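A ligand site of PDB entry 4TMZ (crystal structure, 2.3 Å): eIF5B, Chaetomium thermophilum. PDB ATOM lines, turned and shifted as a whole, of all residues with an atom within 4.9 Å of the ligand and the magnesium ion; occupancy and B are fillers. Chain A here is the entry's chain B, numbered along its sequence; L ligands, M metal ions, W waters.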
ATOM      1  N   GLY A  17      26.064  20.688 -13.982  1.00  0.00           N
ATOM      2  CA  GLY A  17      27.400  20.207 -14.266  1.00  0.00           C
ATOM      3  C   GLY A  17      28.497  21.181 -13.894  1.00  0.00           C
ATOM      4  O   GLY A  17      28.255  22.361 -13.666  1.00  0.00           O
ATOM      5  N   HIS A  18      29.725  20.657 -13.847  1.00  0.00           N
ATOM      6  CA  HIS A  18      30.900  21.452 -13.546  1.00  0.00           C
ATOM      7  C   HIS A  18      31.082  22.496 -14.658  1.00  0.00           C
ATOM      8  O   HIS A  18      30.505  22.362 -15.736  1.00  0.00           O
ATOM      9  CB  HIS A  18      32.135  20.545 -13.417  1.00  0.00           C
ATOM     10  CG  HIS A  18      33.341  21.245 -12.876  1.00  0.00           C
ATOM     11  ND1 HIS A  18      33.517  21.504 -11.535  1.00  0.00           N
ATOM     12  CD2 HIS A  18      34.442  21.727 -13.497  1.00  0.00           C
ATOM     13  CE1 HIS A  18      34.674  22.119 -11.346  1.00  0.00           C
ATOM     14  NE2 HIS A  18      35.262  22.258 -12.515  1.00  0.00           N
ATOM     15  N   VAL A  19      31.863  23.533 -14.372  1.00  0.00           N
ATOM     16  CA  VAL A  19      32.057  24.624 -15.327  1.00  0.00           C
ATOM     17  C   VAL A  19      32.603  24.119 -16.663  1.00  0.00           C
ATOM     18  O   VAL A  19      33.401  23.189 -16.703  1.00  0.00           O
ATOM     19  CB  VAL A  19      32.994  25.715 -14.743  1.00  0.00           C
ATOM     20  CG1 VAL A  19      34.408  25.172 -14.524  1.00  0.00           C
ATOM     21  CG2 VAL A  19      33.016  26.962 -15.633  1.00  0.00           C
ATOM     22  N   ASP A  20      32.130  24.728 -17.757  1.00  0.00           N
ATOM     23  CA  ASP A  20      32.639  24.464 -19.106  1.00  0.00           C
ATOM     24  C   ASP A  20      32.476  23.016 -19.591  1.00  0.00           C
ATOM     25  O   ASP A  20      33.190  22.584 -20.498  1.00  0.00           O
ATOM     26  CB  ASP A  20      34.108  24.858 -19.209  1.00  0.00           C
ATOM     27  CG  ASP A  20      34.305  26.361 -19.352  1.00  0.00           C
ATOM     28  OD1 ASP A  20      35.410  26.850 -19.071  1.00  0.00           O
ATOM     29  OD2 ASP A  20      33.338  27.047 -19.758  1.00  0.00           O
ATOM     30  N   THR A  21      31.531  22.289 -19.011  1.00  0.00           N
ATOM     31  CA  THR A  21      31.315  20.901 -19.429  1.00  0.00           C
ATOM     32  C   THR A  21      30.431  20.805 -20.669  1.00  0.00           C
ATOM     33  O   THR A  21      30.314  19.725 -21.263  1.00  0.00           O
ATOM     34  CB  THR A  21      30.688  20.058 -18.301  1.00  0.00           C
ATOM     35  OG1 THR A  21      29.600  20.774 -17.695  1.00  0.00           O
ATOM     36  CG2 THR A  21      31.727  19.746 -17.235  1.00  0.00           C
ATOM     37  N   GLY A  22      29.818  21.912 -21.077  1.00  0.00           N
ATOM     38  CA  GLY A  22      29.043  21.951 -22.303  1.00  0.00           C
ATOM     39  C   GLY A  22      27.532  21.865 -22.181  1.00  0.00           C
ATOM     40  O   GLY A  22      26.850  21.472 -23.137  1.00  0.00           O
ATOM     41  N   LYS A  23      26.991  22.261 -21.039  1.00  0.00           N
ATOM     42  CA  LYS A  23      25.540  22.269 -20.829  1.00  0.00           C
ATOM     43  C   LYS A  23      24.821  23.151 -21.869  1.00  0.00           C
ATOM     44  O   LYS A  23      23.938  22.688 -22.642  1.00  0.00           O
ATOM     45  CB  LYS A  23      25.235  22.764 -19.408  1.00  0.00           C
ATOM     46  CG  LYS A  23      26.016  22.011 -18.317  1.00  0.00           C
ATOM     47  CD  LYS A  23      25.766  22.583 -16.921  1.00  0.00           C
ATOM     48  CE  LYS A  23      26.515  23.901 -16.707  1.00  0.00           C
ATOM     49  NZ  LYS A  23      27.991  23.729 -16.631  1.00  0.00           N
ATOM     50  N   THR A  24      25.242  24.413 -21.893  1.00  0.00           N
ATOM     51  CA  THR A  24      24.667  25.402 -22.783  1.00  0.00           C
ATOM     52  C   THR A  24      24.927  25.005 -24.224  1.00  0.00           C
ATOM     53  O   THR A  24      24.099  25.224 -25.081  1.00  0.00           O
ATOM     54  CB  THR A  24      25.224  26.799 -22.509  1.00  0.00           C
ATOM     55  OG1 THR A  24      25.015  27.129 -21.128  1.00  0.00           O
ATOM     56  CG2 THR A  24      24.543  27.854 -23.382  1.00  0.00           C
ATOM     57  N   LYS A  25      26.102  24.427 -24.475  1.00  0.00           N
ATOM     58  CA  LYS A  25      26.463  23.984 -25.819  1.00  0.00           C
ATOM     59  C   LYS A  25      25.514  22.890 -26.327  1.00  0.00           C
ATOM     60  O   LYS A  25      25.064  22.922 -27.483  1.00  0.00           O
ATOM     61  CB  LYS A  25      27.898  23.478 -25.836  1.00  0.00           C
ATOM     62  CG  LYS A  25      28.618  23.656 -27.167  1.00  0.00           C
ATOM     63  CD  LYS A  25      28.809  25.123 -27.509  1.00  0.00           C
ATOM     64  CE  LYS A  25      29.490  25.292 -28.859  1.00  0.00           C
ATOM     65  NZ  LYS A  25      29.737  26.723 -29.191  1.00  0.00           N
ATOM     66  N   GLN A  36      25.564  30.297 -26.313  1.00  0.00           N
ATOM     67  CA  GLN A  36      26.864  30.160 -25.664  1.00  0.00           C
ATOM     68  C   GLN A  36      27.865  31.220 -26.120  1.00  0.00           C
ATOM     69  O   GLN A  36      28.580  31.789 -25.285  1.00  0.00           O
ATOM     70  CB  GLN A  36      27.434  28.753 -25.909  1.00  0.00           C
ATOM     71  CG  GLN A  36      28.615  28.392 -25.012  1.00  0.00           C
ATOM     72  CD  GLN A  36      29.955  28.806 -25.587  1.00  0.00           C
ATOM     73  OE1 GLN A  36      30.057  29.208 -26.750  1.00  0.00           O
ATOM     74  NE2 GLN A  36      30.991  28.727 -24.765  1.00  0.00           N
ATOM     75  N   GLU A  39      27.078  34.725 -24.469  1.00  0.00           N
ATOM     76  CA  GLU A  39      27.159  34.930 -23.024  1.00  0.00           C
ATOM     77  C   GLU A  39      28.290  35.885 -22.632  1.00  0.00           C
ATOM     78  O   GLU A  39      29.439  35.705 -23.025  1.00  0.00           O
ATOM     79  CB  GLU A  39      27.345  33.596 -22.305  1.00  0.00           C
ATOM     80  CG  GLU A  39      26.155  32.660 -22.435  1.00  0.00           C
ATOM     81  CD  GLU A  39      26.328  31.388 -21.637  1.00  0.00           C
ATOM     82  OE1 GLU A  39      27.394  30.744 -21.771  1.00  0.00           O
ATOM     83  OE2 GLU A  39      25.397  31.015 -20.898  1.00  0.00           O
ATOM     84  N   GLY A  42      31.860  34.950 -20.986  1.00  0.00           N
ATOM     85  CA  GLY A  42      32.055  33.562 -21.358  1.00  0.00           C
ATOM     86  C   GLY A  42      31.499  32.582 -20.348  1.00  0.00           C
ATOM     87  O   GLY A  42      31.945  31.427 -20.290  1.00  0.00           O
ATOM     88  N   ILE A  43      30.537  33.017 -19.549  1.00  0.00           N
ATOM     89  CA  ILE A  43      29.935  32.137 -18.544  1.00  0.00           C
ATOM     90  C   ILE A  43      28.419  32.256 -18.472  1.00  0.00           C
ATOM     91  O   ILE A  43      27.844  33.297 -18.792  1.00  0.00           O
ATOM     92  CB  ILE A  43      30.502  32.421 -17.140  1.00  0.00           C
ATOM     93  CG1 ILE A  43      30.457  33.926 -16.839  1.00  0.00           C
ATOM     94  CG2 ILE A  43      31.936  31.913 -17.021  1.00  0.00           C
ATOM     95  CD1 ILE A  43      30.730  34.276 -15.389  1.00  0.00           C
ATOM     96  N   THR A  44      27.766  31.180 -18.042  1.00  0.00           N
ATOM     97  CA  THR A  44      26.343  31.204 -17.729  1.00  0.00           C
ATOM     98  C   THR A  44      26.193  31.720 -16.301  1.00  0.00           C
ATOM     99  O   THR A  44      26.818  31.196 -15.389  1.00  0.00           O
ATOM    100  CB  THR A  44      25.705  29.817 -17.865  1.00  0.00           C
ATOM    101  OG1 THR A  44      25.755  29.389 -19.227  1.00  0.00           O
ATOM    102  CG2 THR A  44      24.267  29.834 -17.396  1.00  0.00           C
ATOM    103  N   ASP A  81      18.602  25.374 -18.111  1.00  0.00           N
ATOM    104  CA  ASP A  81      20.051  25.554 -18.082  1.00  0.00           C
ATOM    105  C   ASP A  81      20.463  26.228 -16.782  1.00  0.00           C
ATOM    106  O   ASP A  81      19.778  27.139 -16.301  1.00  0.00           O
ATOM    107  CB  ASP A  81      20.513  26.382 -19.283  1.00  0.00           C
ATOM    108  CG  ASP A  81      21.985  26.180 -19.607  1.00  0.00           C
ATOM    109  OD1 ASP A  81      22.648  25.385 -18.917  1.00  0.00           O
ATOM    110  OD2 ASP A  81      22.465  26.816 -20.564  1.00  0.00           O
ATOM    111  N   THR A  82      21.583  25.791 -16.219  1.00  0.00           N
ATOM    112  CA  THR A  82      22.085  26.336 -14.956  1.00  0.00           C
ATOM    113  C   THR A  82      23.573  26.648 -15.058  1.00  0.00           C
ATOM    114  O   THR A  82      24.280  26.056 -15.864  1.00  0.00           O
ATOM    115  CB  THR A  82      21.840  25.354 -13.778  1.00  0.00           C
ATOM    116  OG1 THR A  82      22.586  24.152 -13.981  1.00  0.00           O
ATOM    117  CG2 THR A  82      20.364  25.035 -13.623  1.00  0.00           C
ATOM    118  N   PRO A  83      24.053  27.593 -14.224  1.00  0.00           N
ATOM    119  CA  PRO A  83      25.479  27.913 -14.186  1.00  0.00           C
ATOM    120  C   PRO A  83      26.330  26.762 -13.639  1.00  0.00           C
ATOM    121  O   PRO A  83      25.880  26.049 -12.744  1.00  0.00           O
ATOM    122  CB  PRO A  83      25.542  29.129 -13.250  1.00  0.00           C
ATOM    123  CG  PRO A  83      24.164  29.703 -13.279  1.00  0.00           C
ATOM    124  CD  PRO A  83      23.270  28.497 -13.377  1.00  0.00           C
ATOM    125  N   GLY A  84      27.533  26.597 -14.170  1.00  0.00           N
ATOM    126  CA  GLY A  84      28.454  25.585 -13.686  1.00  0.00           C
ATOM    127  C   GLY A  84      29.560  26.107 -12.784  1.00  0.00           C
ATOM    128  O   GLY A  84      30.166  25.344 -12.025  1.00  0.00           O
ATOM    129  N   HIS A  85      29.838  27.402 -12.845  1.00  0.00           N
ATOM    130  CA  HIS A  85      30.919  27.988 -12.058  1.00  0.00           C
ATOM    131  C   HIS A  85      30.620  27.863 -10.561  1.00  0.00           C
ATOM    132  O   HIS A  85      29.469  27.909 -10.138  1.00  0.00           O
ATOM    133  CB  HIS A  85      31.139  29.456 -12.446  1.00  0.00           C
ATOM    134  CG  HIS A  85      32.398  30.035 -11.890  1.00  0.00           C
ATOM    135  ND1 HIS A  85      32.504  30.488 -10.585  1.00  0.00           N
ATOM    136  CD2 HIS A  85      33.606  30.240 -12.457  1.00  0.00           C
ATOM    137  CE1 HIS A  85      33.730  30.943 -10.384  1.00  0.00           C
ATOM    138  NE2 HIS A  85      34.414  30.807 -11.500  1.00  0.00           N
ATOM    139  N   ASN A 135      29.814  14.067 -22.038  1.00  0.00           N
ATOM    140  CA  ASN A 135      29.970  14.985 -23.161  1.00  0.00           C
ATOM    141  C   ASN A 135      31.389  15.053 -23.695  1.00  0.00           C
ATOM    142  O   ASN A 135      32.332  14.594 -23.064  1.00  0.00           O
ATOM    143  CB  ASN A 135      29.502  16.377 -22.735  1.00  0.00           C
ATOM    144  CG  ASN A 135      29.227  17.291 -23.913  1.00  0.00           C
ATOM    145  OD1 ASN A 135      28.765  16.835 -24.962  1.00  0.00           O
ATOM    146  ND2 ASN A 135      29.500  18.581 -23.746  1.00  0.00           N
ATOM    147  N   LYS A 136      31.521  15.628 -24.900  1.00  0.00           N
ATOM    148  CA  LYS A 136      32.792  15.862 -25.588  1.00  0.00           C
ATOM    149  C   LYS A 136      33.500  14.570 -26.021  1.00  0.00           C
ATOM    150  O   LYS A 136      34.717  14.465 -25.929  1.00  0.00           O
ATOM    151  CB  LYS A 136      33.731  16.700 -24.708  1.00  0.00           C
ATOM    152  CG  LYS A 136      33.079  17.907 -24.048  1.00  0.00           C
ATOM    153  CD  LYS A 136      34.104  18.844 -23.441  1.00  0.00           C
ATOM    154  CE  LYS A 136      33.457  20.148 -22.993  1.00  0.00           C
ATOM    155  NZ  LYS A 136      34.435  21.098 -22.401  1.00  0.00           N
ATOM    156  N   ASP A 138      33.816  13.703 -28.970  1.00  0.00           N
ATOM    157  CA  ASP A 138      34.564  14.061 -30.187  1.00  0.00           C
ATOM    158  C   ASP A 138      36.039  14.321 -29.859  1.00  0.00           C
ATOM    159  O   ASP A 138      36.866  14.424 -30.761  1.00  0.00           O
ATOM    160  CB  ASP A 138      33.958  15.292 -30.867  1.00  0.00           C
ATOM    161  CG  ASP A 138      33.923  16.507 -29.959  1.00  0.00           C
ATOM    162  OD1 ASP A 138      34.840  17.351 -30.057  1.00  0.00           O
ATOM    163  OD2 ASP A 138      32.995  16.609 -29.149  1.00  0.00           O
ATOM    164  N   ARG A 139      36.344  14.416 -28.574  1.00  0.00           N
ATOM    165  CA  ARG A 139      37.701  14.691 -28.128  1.00  0.00           C
ATOM    166  C   ARG A 139      38.497  13.398 -27.946  1.00  0.00           C
ATOM    167  O   ARG A 139      39.690  13.434 -27.638  1.00  0.00           O
ATOM    168  CB  ARG A 139      37.686  15.470 -26.811  1.00  0.00           C
ATOM    169  CG  ARG A 139      37.115  16.862 -26.909  1.00  0.00           C
ATOM    170  CD  ARG A 139      38.090  17.812 -27.556  1.00  0.00           C
ATOM    171  NE  ARG A 139      39.227  18.086 -26.677  1.00  0.00           N
ATOM    172  CZ  ARG A 139      40.343  18.704 -27.075  1.00  0.00           C
ATOM    173  NH1 ARG A 139      41.329  18.906 -26.206  1.00  0.00           N
ATOM    174  NH2 ARG A 139      40.471  19.120 -28.328  1.00  0.00           N
ATOM    175  N   THR A 202      27.907  11.727 -25.243  1.00  0.00           N
ATOM    176  CA  THR A 202      27.401  12.748 -26.153  1.00  0.00           C
ATOM    177  C   THR A 202      28.494  13.672 -26.667  1.00  0.00           C
ATOM    178  O   THR A 202      29.562  13.779 -26.081  1.00  0.00           O
ATOM    179  CB  THR A 202      26.305  13.618 -25.494  1.00  0.00           C
ATOM    180  OG1 THR A 202      26.873  14.368 -24.412  1.00  0.00           O
ATOM    181  CG2 THR A 202      25.139  12.777 -24.967  1.00  0.00           C
ATOM    182  N   SER A 203      28.206  14.339 -27.781  1.00  0.00           N
ATOM    183  CA  SER A 203      29.021  15.455 -28.239  1.00  0.00           C
ATOM    184  C   SER A 203      28.132  16.656 -28.558  1.00  0.00           C
ATOM    185  O   SER A 203      27.250  16.561 -29.411  1.00  0.00           O
ATOM    186  CB  SER A 203      29.841  15.059 -29.470  1.00  0.00           C
ATOM    187  OG  SER A 203      30.604  16.153 -29.935  1.00  0.00           O
ATOM    188  N   ALA A 204      28.364  17.772 -27.885  1.00  0.00           N
ATOM    189  CA  ALA A 204      27.602  18.985 -28.157  1.00  0.00           C
ATOM    190  C   ALA A 204      27.984  19.583 -29.506  1.00  0.00           C
ATOM    191  O   ALA A 204      27.194  20.293 -30.116  1.00  0.00           O
ATOM    192  CB  ALA A 204      27.814  20.009 -27.037  1.00  0.00           C
ATOM    193  N   HIS A 205      29.209  19.296 -29.961  1.00  0.00           N
ATOM    194  CA  HIS A 205      29.671  19.799 -31.249  1.00  0.00           C
ATOM    195  C   HIS A 205      29.091  19.012 -32.423  1.00  0.00           C
ATOM    196  O   HIS A 205      28.627  19.610 -33.387  1.00  0.00           O
ATOM    197  CB  HIS A 205      31.199  19.779 -31.311  1.00  0.00           C
ATOM    198  CG  HIS A 205      31.855  20.916 -30.584  1.00  0.00           C
ATOM    199  ND1 HIS A 205      33.204  21.130 -30.608  1.00  0.00           N
ATOM    200  CD2 HIS A 205      31.319  21.903 -29.814  1.00  0.00           C
ATOM    201  CE1 HIS A 205      33.495  22.212 -29.881  1.00  0.00           C
ATOM    202  NE2 HIS A 205      32.372  22.685 -29.394  1.00  0.00           N
HETATM  203  P1  LIG L   1      29.192  27.004 -17.812  1.00  0.00           P
HETATM  204  O1  LIG L   1      29.696  26.228 -19.115  1.00  0.00           O
HETATM  205  S1  LIG L   1      30.190  28.667 -17.712  1.00  0.00           S
HETATM  206  O2  LIG L   1      29.463  26.133 -16.501  1.00  0.00           O
HETATM  207  O3  LIG L   1      27.631  27.322 -17.930  1.00  0.00           O
HETATM  208  P2  LIG L   1      28.821  25.149 -19.891  1.00  0.00           P
HETATM  209  O4  LIG L   1      27.515  25.778 -20.264  1.00  0.00           O
HETATM  210  O5  LIG L   1      28.833  23.878 -19.109  1.00  0.00           O
HETATM  211  P3  LIG L   1      29.650  25.766 -22.529  1.00  0.00           P
HETATM  212  O6  LIG L   1      29.877  27.212 -22.192  1.00  0.00           O
HETATM  213  O7  LIG L   1      28.423  25.352 -23.284  1.00  0.00           O
HETATM  214  O8  LIG L   1      29.710  24.883 -21.191  1.00  0.00           O
HETATM  215  O9  LIG L   1      30.933  25.235 -23.311  1.00  0.00           O
HETATM  216  C1  LIG L   1      32.224  25.291 -22.697  1.00  0.00           C
HETATM  217  C2  LIG L   1      33.297  25.137 -23.762  1.00  0.00           C
HETATM  218  O10 LIG L   1      33.466  23.762 -24.089  1.00  0.00           O
HETATM  219  C3  LIG L   1      32.920  25.860 -25.043  1.00  0.00           C
HETATM  220  O11 LIG L   1      34.077  26.473 -25.585  1.00  0.00           O
HETATM  221  C4  LIG L   1      32.465  24.764 -25.980  1.00  0.00           C
HETATM  222  O12 LIG L   1      32.837  25.070 -27.319  1.00  0.00           O
HETATM  223  C5  LIG L   1      33.213  23.548 -25.480  1.00  0.00           C
HETATM  224  N1  LIG L   1      32.401  22.327 -25.666  1.00  0.00           N
HETATM  225  C6  LIG L   1      31.187  22.100 -25.149  1.00  0.00           C
HETATM  226  N2  LIG L   1      30.722  20.878 -25.528  1.00  0.00           N
HETATM  227  C7  LIG L   1      31.662  20.319 -26.294  1.00  0.00           C
HETATM  228  C8  LIG L   1      31.814  19.038 -27.023  1.00  0.00           C
HETATM  229  O13 LIG L   1      30.915  18.181 -26.986  1.00  0.00           O
HETATM  230  N3  LIG L   1      32.945  18.848 -27.705  1.00  0.00           N
HETATM  231  C9  LIG L   1      33.924  19.765 -27.748  1.00  0.00           C
HETATM  232  N4  LIG L   1      35.038  19.483 -28.463  1.00  0.00           N
HETATM  233  N5  LIG L   1      33.855  20.952 -27.109  1.00  0.00           N
HETATM  234  C10 LIG L   1      32.767  21.280 -26.386  1.00  0.00           C
HETATM  235 MG    MG M   1      26.498  27.348 -19.694  1.00  0.00          MG
HETATM  236  O   HOH W   1      24.986  26.428 -18.454  1.00  0.00           O
HETATM  237  O   HOH W   2      28.872  29.339 -14.996  1.00  0.00           O
HETATM  238  O   HOH W   3      27.884  28.343 -20.913  1.00  0.00           O
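An oxygen (O5) of the ligand is in salt-bridge range of the side-chain amino group (NZ) of Lys 23, at 2.6 Å.
O4 of the ligand sits close to N of Thr 24.
O2 of the ligand sits close to N of Gly 84 (3.1 Å).
The side-chain hydroxyl of Thr 21 lies within hydrogen-bond range of an oxygen (O5) of the ligand (3.5 Å).
The backbone NH (N) of Thr 21 is in hydrogen-bond range of an oxygen (O5) of the ligand (3.1 Å).
NZ of Lys 136 lies within hydrogen-bond range of O10 of the ligand (3.3 Å).
N of Asp 20 sits at hydrogen-bond distance from O1 of the ligand.
The side-chain amide nitrogen of Gln 36 lies within hydrogen-bond range of an oxygen (O6) of the ligand (3.2 Å).
OD2 of Asp 138 is in hydrogen-bond range of N3 of the ligand, 2.7 Å away.
The backbone NH (N) of Lys 136 lies close to an oxygen (O13) of the ligand (3.4 Å).
The side-chain amide nitrogen (ND2) of Asn 135 sits at hydrogen-bond distance from a nitrogen (N2) of the ligand, 3.2 Å away.
N of Ala 204 sits at hydrogen-bond distance from O13 of the ligand, 2.7 Å away.
The backbone NH (N) of Gly 22 sits at hydrogen-bond distance from an oxygen (O5) of the ligand (3.0 Å).
An oxygen (O7) of the ligand sits at hydrogen-bond distance from the backbone NH of Lys 25 (2.8 Å).
A ring nitrogen (NE2) of His 205 is in hydrogen-bond range of an oxygen (O12) of the ligand.
An oxygen (O5) of the ligand sits at hydrogen-bond distance from the backbone NH (N) of Lys 23 (3.1 Å).
S1 of the ligand sits close to N of Thr 44.
NZ of Lys 23 sits at hydrogen-bond distance from O of Gly 17 (3.3 Å).
The side-chain amino group (NZ) of Lys 25 is in hydrogen-bond range of the side-chain amide oxygen (OE1) of Gln 36 (3.5 Å).
N of Lys 136 is in hydrogen-bond range of O of Thr 202.
OE1 of Glu 39 lies close to OG1 of Thr 44.
OG1 of Thr 24 lies close to OD2 of Asp 81 (2.6 Å).
The backbone carbonyl oxygen of His 18 lies within hydrogen-bond range of the side-chain hydroxyl of Thr 21 (2.7 Å).
OD1 of Asn 135 sits at hydrogen-bond distance from N of Ala 204.
The side-chain amino group (NZ) of Lys 23 lies within hydrogen-bond range of the backbone carbonyl oxygen (O) of His 18, at 3.0 Å.
Residues that only touch the ligand: Val 19, Ser 203, Ile 43, Arg 139, His 85 and His 18.
Hydrophobic or aromatic side chains that line the ligand: Val 19, Ile 43, Ala 204 and His 205.
The nearest printed residue that does not touch the ligand is Thr 82 (4.1 Å).
Of the 27 residues printed, 2 come within 4 Å of the magnesium ion.
The magnesium ion is bound by O4 of the ligand, OG1 of Thr 24, O3 of the ligand, water W3, water W1 and OG1 of Thr 44.
Water W3 lies within hydrogen-bond range of OE1 of Glu 39 (2.6 Å) and O6 of the ligand (2.6 Å).
Water W1 bridges OD1 of Asp 81 and O of Thr 82.
Water W2 lies within hydrogen-bond range of the backbone carbonyl oxygen of Thr 44 (2.8 Å), the backbone NH of His 85 (3.1 Å), a sulfur (S1) of the ligand (3.1 Å) and the backbone NH of Gly 84 (3.2 Å).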
